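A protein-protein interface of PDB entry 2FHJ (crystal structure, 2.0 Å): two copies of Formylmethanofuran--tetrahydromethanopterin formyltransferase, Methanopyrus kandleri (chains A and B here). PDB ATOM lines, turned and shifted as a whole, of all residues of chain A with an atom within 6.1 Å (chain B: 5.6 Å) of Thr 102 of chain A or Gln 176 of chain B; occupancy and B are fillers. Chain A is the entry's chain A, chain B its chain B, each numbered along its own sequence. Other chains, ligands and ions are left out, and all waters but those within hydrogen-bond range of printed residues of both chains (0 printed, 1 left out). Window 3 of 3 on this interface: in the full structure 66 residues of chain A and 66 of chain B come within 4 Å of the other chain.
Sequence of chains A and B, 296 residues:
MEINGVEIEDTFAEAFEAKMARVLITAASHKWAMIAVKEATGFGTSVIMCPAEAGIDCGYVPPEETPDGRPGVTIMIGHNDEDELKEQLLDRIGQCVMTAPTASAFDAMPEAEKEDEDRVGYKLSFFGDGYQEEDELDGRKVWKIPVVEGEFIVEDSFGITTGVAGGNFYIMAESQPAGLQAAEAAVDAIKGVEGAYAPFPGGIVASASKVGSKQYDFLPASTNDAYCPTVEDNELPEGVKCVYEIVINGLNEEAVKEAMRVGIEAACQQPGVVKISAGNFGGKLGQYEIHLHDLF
No position is printed for both chains.
Thr 26 of chain A touches none of the printed residues of chain B.
Ala 28 of chain A touches none of the printed residues of chain B.
Of the printed residues of chain B, Trp 32 of chain A touches Leu 180.
Of the printed residues of chain B, Pro 101 of chain A touches Leu 180 and Ala 206.
Of chain B, only Gln 176, Leu 180 and Tyr 244 come within 4 Å of Thr 102 of chain A.
Printed residues of chain B within 4 Å of Glu 149 of chain A: Ala 206, Cys 242 and Tyr 244.
Printed residues of chain A within 4 Å of Gln 176 of chain B: Thr 102 (3.4 Å).
Of the printed residues of chain A, Leu 180 of chain B touches Trp 32, Pro 101 and Thr 102.
Printed residues of chain A within 4 Å of Tyr 244 of chain B: Thr 102 and Glu 149.
The nearest printed residue of chain A that does not touch Gln 176 of chain B is Glu 149 of chain A (4.01 Å).
The backbone carbonyl oxygen (O) of Ala 206 of chain B lies within hydrogen-bond range of the backbone NH (N) of Glu 149 of chain A (3.2 Å).
O of Glu 149 of chain A sits at hydrogen-bond distance from SG of Cys 242 of chain B (3.6 Å).
OE1 of Glu 149 of chain A lies within hydrogen-bond range of OH of Tyr 244 of chain B (2.5 Å).
The backbone NH (N) of Ala 28 of chain A sits at hydrogen-bond distance from the side-chain hydroxyl (OG1) of Thr 102 of chain A.
The side-chain hydroxyl (OG) of Ser 29 of chain A lies close to the backbone NH (N) of Trp 32 of chain A.
The guanidinium group (NH1) of Arg 70 of chain A lies within hydrogen-bond range of the backbone carbonyl oxygen (O) of Thr 102 of chain A (2.8 Å).
The backbone NH (N) of Thr 102 of chain A is in hydrogen-bond range of the side-chain carboxylate (OE1) of Glu 149 of chain A (2.6 Å).
Printed residues of chain A that touch a printed residue of chain B: Trp 32, Ala 100, Pro 101, Thr 102 and Glu 149.
Printed residues of chain B that touch a printed residue of chain A: Gln 176, Leu 180, Ala 206, Cys 242 and Tyr 244.
Hydrophobic or aromatic side chains of chain B within 4 Å of the printed part of chain A: Leu 180, Ala 206 and Tyr 244.
CE2 of Trp 32 of chain A touches CD2 of Leu 180 of chain B, 3.7 Å away.
O of Ala 100 of chain A touches CB of Ala 206 of chain B, at 3.8 Å.
Pro 101 of chain A touches Leu 180 of chain B.
Ala 206 of chain B touches Pro 101 of chain A.
Gln 176 of chain B touches Thr 102 of chain A (NE2 to CG2, 3.4 Å).
CG2 of Thr 102 of chain A touches CD2 of Leu 180 of chain B, at 3.6 Å.
OH of Tyr 244 of chain B touches CG2 of Thr 102 of chain A, 3.9 Å away.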
ATOM      1  N   THR A  26      16.232  22.530  -1.627  1.00  0.00           N
ATOM      2  CA  THR A  26      17.184  22.859  -0.581  1.00  0.00           C
ATOM      3  C   THR A  26      16.385  22.995   0.712  1.00  0.00           C
ATOM      4  O   THR A  26      15.144  23.154   0.680  1.00  0.00           O
ATOM      5  CB  THR A  26      17.960  24.146  -0.896  1.00  0.00           C
ATOM      6  OG1 THR A  26      17.056  25.252  -0.948  1.00  0.00           O
ATOM      7  CG2 THR A  26      18.675  24.022  -2.230  1.00  0.00           C
ATOM      8  N   ALA A  27      17.086  22.891   1.839  1.00  0.00           N
ATOM      9  CA  ALA A  27      16.490  23.063   3.145  1.00  0.00           C
ATOM     10  C   ALA A  27      17.595  23.448   4.098  1.00  0.00           C
ATOM     11  O   ALA A  27      18.713  23.609   3.670  1.00  0.00           O
ATOM     12  CB  ALA A  27      15.840  21.797   3.580  1.00  0.00           C
ATOM     13  N   ALA A  28      17.268  23.625   5.374  1.00  0.00           N
ATOM     14  CA  ALA A  28      18.267  24.004   6.384  1.00  0.00           C
ATOM     15  C   ALA A  28      19.314  22.932   6.625  1.00  0.00           C
ATOM     16  O   ALA A  28      20.391  23.228   7.112  1.00  0.00           O
ATOM     17  CB  ALA A  28      17.594  24.340   7.690  1.00  0.00           C
ATOM     18  N   SER A  29      18.959  21.687   6.345  1.00  0.00           N
ATOM     19  CA  SER A  29      19.880  20.566   6.463  1.00  0.00           C
ATOM     20  C   SER A  29      19.547  19.527   5.411  1.00  0.00           C
ATOM     21  O   SER A  29      18.480  19.577   4.788  1.00  0.00           O
ATOM     22  CB  SER A  29      19.774  19.928   7.852  1.00  0.00           C
ATOM     23  OG  SER A  29      18.448  19.495   8.124  1.00  0.00           O
ATOM     24  N   TRP A  32      16.231  17.869   6.599  1.00  0.00           N
ATOM     25  CA  TRP A  32      14.941  18.502   6.236  1.00  0.00           C
ATOM     26  C   TRP A  32      14.689  18.495   4.758  1.00  0.00           C
ATOM     27  O   TRP A  32      13.537  18.461   4.326  1.00  0.00           O
ATOM     28  CB  TRP A  32      14.808  19.916   6.794  1.00  0.00           C
ATOM     29  CG  TRP A  32      14.696  19.894   8.282  1.00  0.00           C
ATOM     30  CD1 TRP A  32      15.653  20.253   9.175  1.00  0.00           C
ATOM     31  CD2 TRP A  32      13.591  19.415   9.043  1.00  0.00           C
ATOM     32  NE1 TRP A  32      15.202  20.057  10.459  1.00  0.00           N
ATOM     33  CE2 TRP A  32      13.938  19.534  10.403  1.00  0.00           C
ATOM     34  CE3 TRP A  32      12.336  18.894   8.710  1.00  0.00           C
ATOM     35  CZ2 TRP A  32      13.081  19.153  11.420  1.00  0.00           C
ATOM     36  CZ3 TRP A  32      11.492  18.519   9.722  1.00  0.00           C
ATOM     37  CH2 TRP A  32      11.853  18.665  11.057  1.00  0.00           C
ATOM     38  N   ALA A  33      15.762  18.536   3.973  1.00  0.00           N
ATOM     39  CA  ALA A  33      15.674  18.370   2.515  1.00  0.00           C
ATOM     40  C   ALA A  33      15.052  17.011   2.167  1.00  0.00           C
ATOM     41  O   ALA A  33      14.125  16.927   1.352  1.00  0.00           O
ATOM     42  CB  ALA A  33      17.079  18.531   1.879  1.00  0.00           C
ATOM     43  N   ARG A  70      22.623  26.393   0.640  1.00  0.00           N
ATOM     44  CA  ARG A  70      22.100  25.425   1.602  1.00  0.00           C
ATOM     45  C   ARG A  70      22.135  24.011   1.033  1.00  0.00           C
ATOM     46  O   ARG A  70      22.128  23.843  -0.194  1.00  0.00           O
ATOM     47  CB  ARG A  70      20.646  25.761   1.936  1.00  0.00           C
ATOM     48  CG  ARG A  70      20.435  27.171   2.458  1.00  0.00           C
ATOM     49  CD  ARG A  70      19.143  27.293   3.199  1.00  0.00           C
ATOM     50  NE  ARG A  70      18.008  26.986   2.327  1.00  0.00           N
ATOM     51  CZ  ARG A  70      16.794  26.674   2.754  1.00  0.00           C
ATOM     52  NH1 ARG A  70      15.837  26.416   1.867  1.00  0.00           N
ATOM     53  NH2 ARG A  70      16.533  26.606   4.049  1.00  0.00           N
ATOM     54  N   ALA A 100       6.863  21.928   3.887  1.00  0.00           N
ATOM     55  CA  ALA A 100       7.937  21.250   4.616  1.00  0.00           C
ATOM     56  C   ALA A 100       8.839  22.251   5.277  1.00  0.00           C
ATOM     57  O   ALA A 100       9.272  23.208   4.648  1.00  0.00           O
ATOM     58  CB  ALA A 100       8.745  20.353   3.694  1.00  0.00           C
ATOM     59  N   PRO A 101       9.154  22.031   6.553  1.00  0.00           N
ATOM     60  CA  PRO A 101      10.058  22.964   7.200  1.00  0.00           C
ATOM     61  C   PRO A 101      11.294  23.343   6.369  1.00  0.00           C
ATOM     62  O   PRO A 101      12.013  22.475   5.864  1.00  0.00           O
ATOM     63  CB  PRO A 101      10.442  22.230   8.473  1.00  0.00           C
ATOM     64  CG  PRO A 101       9.205  21.482   8.811  1.00  0.00           C
ATOM     65  CD  PRO A 101       8.701  20.984   7.485  1.00  0.00           C
ATOM     66  N   THR A 102      11.459  24.656   6.216  1.00  0.00           N
ATOM     67  CA  THR A 102      12.625  25.323   5.680  1.00  0.00           C
ATOM     68  C   THR A 102      12.931  25.084   4.222  1.00  0.00           C
ATOM     69  O   THR A 102      13.898  25.628   3.727  1.00  0.00           O
ATOM     70  CB  THR A 102      13.884  24.954   6.481  1.00  0.00           C
ATOM     71  OG1 THR A 102      14.326  23.643   6.120  1.00  0.00           O
ATOM     72  CG2 THR A 102      13.603  25.009   7.956  1.00  0.00           C
ATOM     73  N   ALA A 103      12.147  24.272   3.522  1.00  0.00           N
ATOM     74  CA  ALA A 103      12.547  23.853   2.173  1.00  0.00           C
ATOM     75  C   ALA A 103      12.169  24.837   1.059  1.00  0.00           C
ATOM     76  O   ALA A 103      11.115  25.475   1.106  1.00  0.00           O
ATOM     77  CB  ALA A 103      12.026  22.451   1.880  1.00  0.00           C
ATOM     78  N   SER A 104      13.063  24.965   0.079  1.00  0.00           N
ATOM     79  CA  SER A 104      12.876  25.823  -1.095  1.00  0.00           C
ATOM     80  C   SER A 104      12.964  24.934  -2.327  1.00  0.00           C
ATOM     81  O   SER A 104      13.523  23.849  -2.251  1.00  0.00           O
ATOM     82  CB  SER A 104      13.959  26.896  -1.157  1.00  0.00           C
ATOM     83  OG  SER A 104      14.066  27.624   0.058  1.00  0.00           O
ATOM     84  N   GLU A 149       6.025  30.222   8.598  1.00  0.00           N
ATOM     85  CA  GLU A 149       7.429  29.988   8.964  1.00  0.00           C
ATOM     86  C   GLU A 149       8.266  31.225   8.654  1.00  0.00           C
ATOM     87  O   GLU A 149       9.256  31.491   9.314  1.00  0.00           O
ATOM     88  CB  GLU A 149       7.980  28.781   8.189  1.00  0.00           C
ATOM     89  CG  GLU A 149       9.441  28.432   8.496  1.00  0.00           C
ATOM     90  CD  GLU A 149      10.026  27.472   7.476  1.00  0.00           C
ATOM     91  OE1 GLU A 149      10.363  26.338   7.856  1.00  0.00           O
ATOM     92  OE2 GLU A 149      10.128  27.850   6.294  1.00  0.00           O
ATOM     93  N   GLU B 174      10.528  32.682  18.863  1.00  0.00           N
ATOM     94  CA  GLU B 174      11.380  33.847  18.665  1.00  0.00           C
ATOM     95  C   GLU B 174      12.124  33.841  17.330  1.00  0.00           C
ATOM     96  O   GLU B 174      12.658  34.875  16.923  1.00  0.00           O
ATOM     97  CB  GLU B 174      12.388  33.955  19.809  1.00  0.00           C
ATOM     98  CG  GLU B 174      13.396  32.809  19.805  1.00  0.00           C
ATOM     99  CD  GLU B 174      14.452  32.927  20.889  1.00  0.00           C
ATOM    100  OE1 GLU B 174      14.203  33.629  21.902  1.00  0.00           O
ATOM    101  OE2 GLU B 174      15.525  32.303  20.722  1.00  0.00           O
ATOM    102  N   SER B 175      12.183  32.675  16.669  1.00  0.00           N
ATOM    103  CA  SER B 175      12.876  32.517  15.383  1.00  0.00           C
ATOM    104  C   SER B 175      12.456  31.219  14.683  1.00  0.00           C
ATOM    105  O   SER B 175      11.741  30.403  15.259  1.00  0.00           O
ATOM    106  CB  SER B 175      14.379  32.466  15.638  1.00  0.00           C
ATOM    107  OG  SER B 175      14.657  31.284  16.334  1.00  0.00           O
ATOM    108  N   GLN B 176      12.912  31.027  13.447  1.00  0.00           N
ATOM    109  CA  GLN B 176      12.693  29.756  12.732  1.00  0.00           C
ATOM    110  C   GLN B 176      13.468  28.590  13.361  1.00  0.00           C
ATOM    111  O   GLN B 176      12.896  27.563  13.655  1.00  0.00           O
ATOM    112  CB  GLN B 176      12.998  29.901  11.246  1.00  0.00           C
ATOM    113  CG  GLN B 176      12.948  28.614  10.426  1.00  0.00           C
ATOM    114  CD  GLN B 176      14.271  27.871  10.410  1.00  0.00           C
ATOM    115  OE1 GLN B 176      15.285  28.409   9.988  1.00  0.00           O
ATOM    116  NE2 GLN B 176      14.267  26.643  10.882  1.00  0.00           N
ATOM    117  N   PRO B 177      14.780  28.730  13.576  1.00  0.00           N
ATOM    118  CA  PRO B 177      15.408  27.575  14.228  1.00  0.00           C
ATOM    119  C   PRO B 177      14.720  27.107  15.517  1.00  0.00           C
ATOM    120  O   PRO B 177      14.604  25.898  15.764  1.00  0.00           O
ATOM    121  CB  PRO B 177      16.839  28.066  14.501  1.00  0.00           C
ATOM    122  CG  PRO B 177      17.084  29.099  13.481  1.00  0.00           C
ATOM    123  CD  PRO B 177      15.754  29.773  13.229  1.00  0.00           C
ATOM    124  N   ALA B 178      14.257  28.046  16.333  1.00  0.00           N
ATOM    125  CA  ALA B 178      13.669  27.715  17.614  1.00  0.00           C
ATOM    126  C   ALA B 178      12.295  27.079  17.455  1.00  0.00           C
ATOM    127  O   ALA B 178      11.955  26.150  18.175  1.00  0.00           O
ATOM    128  CB  ALA B 178      13.588  28.973  18.490  1.00  0.00           C
ATOM    129  N   GLY B 179      11.496  27.585  16.524  1.00  0.00           N
ATOM    130  CA  GLY B 179      10.175  26.997  16.245  1.00  0.00           C
ATOM    131  C   GLY B 179      10.237  25.567  15.742  1.00  0.00           C
ATOM    132  O   GLY B 179       9.378  24.745  16.068  1.00  0.00           O
ATOM    133  N   LEU B 180      11.266  25.269  14.946  1.00  0.00           N
ATOM    134  CA  LEU B 180      11.470  23.942  14.395  1.00  0.00           C
ATOM    135  C   LEU B 180      12.077  22.975  15.416  1.00  0.00           C
ATOM    136  O   LEU B 180      11.735  21.810  15.408  1.00  0.00           O
ATOM    137  CB  LEU B 180      12.339  24.004  13.143  1.00  0.00           C
ATOM    138  CG  LEU B 180      12.376  22.754  12.256  1.00  0.00           C
ATOM    139  CD1 LEU B 180      10.971  22.243  11.942  1.00  0.00           C
ATOM    140  CD2 LEU B 180      13.127  23.071  10.981  1.00  0.00           C
ATOM    141  N   GLN B 181      12.994  23.420  16.277  1.00  0.00           N
ATOM    142  CA  GLN B 181      13.449  22.549  17.359  1.00  0.00           C
ATOM    143  C   GLN B 181      12.257  22.166  18.237  1.00  0.00           C
ATOM    144  O   GLN B 181      12.152  21.030  18.677  1.00  0.00           O
ATOM    145  CB  GLN B 181      14.565  23.187  18.197  1.00  0.00           C
ATOM    146  CG  GLN B 181      15.123  22.246  19.238  1.00  0.00           C
ATOM    147  CD  GLN B 181      16.398  22.734  19.896  1.00  0.00           C
ATOM    148  OE1 GLN B 181      17.396  22.994  19.230  1.00  0.00           O
ATOM    149  NE2 GLN B 181      16.378  22.822  21.217  1.00  0.00           N
ATOM    150  N   ALA B 206       4.826  24.276   7.530  1.00  0.00           N
ATOM    151  CA  ALA B 206       5.559  25.532   7.498  1.00  0.00           C
ATOM    152  C   ALA B 206       4.750  26.612   6.811  1.00  0.00           C
ATOM    153  O   ALA B 206       5.153  27.781   6.798  1.00  0.00           O
ATOM    154  CB  ALA B 206       6.900  25.353   6.771  1.00  0.00           C
ATOM    155  N   LYS B 241       8.913  35.619  15.399  1.00  0.00           N
ATOM    156  CA  LYS B 241       9.449  35.714  14.040  1.00  0.00           C
ATOM    157  C   LYS B 241       9.151  34.477  13.181  1.00  0.00           C
ATOM    158  O   LYS B 241       9.436  34.468  11.982  1.00  0.00           O
ATOM    159  CB  LYS B 241      10.956  35.946  14.105  1.00  0.00           C
ATOM    160  CG  LYS B 241      11.363  37.118  15.015  1.00  0.00           C
ATOM    161  CD  LYS B 241      12.890  37.296  15.057  1.00  0.00           C
ATOM    162  CE  LYS B 241      13.338  38.679  14.589  1.00  0.00           C
ATOM    163  NZ  LYS B 241      12.355  39.350  13.679  1.00  0.00           N
ATOM    164  N   CYS B 242       8.564  33.445  13.793  1.00  0.00           N
ATOM    165  CA  CYS B 242       8.270  32.183  13.106  1.00  0.00           C
ATOM    166  C   CYS B 242       7.099  31.461  13.747  1.00  0.00           C
ATOM    167  O   CYS B 242       7.032  31.345  14.967  1.00  0.00           O
ATOM    168  CB  CYS B 242       9.485  31.248  13.151  1.00  0.00           C
ATOM    169  SG  CYS B 242       9.222  29.650  12.350  1.00  0.00           S
ATOM    170  N   TYR B 244       4.901  27.715  13.373  1.00  0.00           N
ATOM    171  CA  TYR B 244       4.730  26.383  12.786  1.00  0.00           C
ATOM    172  C   TYR B 244       3.427  25.811  13.280  1.00  0.00           C
ATOM    173  O   TYR B 244       3.080  26.006  14.427  1.00  0.00           O
ATOM    174  CB  TYR B 244       5.854  25.440  13.218  1.00  0.00           C
ATOM    175  CG  TYR B 244       7.119  25.583  12.440  1.00  0.00           C
ATOM    176  CD1 TYR B 244       8.279  26.074  13.044  1.00  0.00           C
ATOM    177  CD2 TYR B 244       7.188  25.199  11.099  1.00  0.00           C
ATOM    178  CE1 TYR B 244       9.473  26.189  12.325  1.00  0.00           C
ATOM    179  CE2 TYR B 244       8.373  25.315  10.369  1.00  0.00           C
ATOM    180  CZ  TYR B 244       9.512  25.794  10.999  1.00  0.00           C
ATOM    181  OH  TYR B 244      10.669  25.920  10.278  1.00  0.00           O
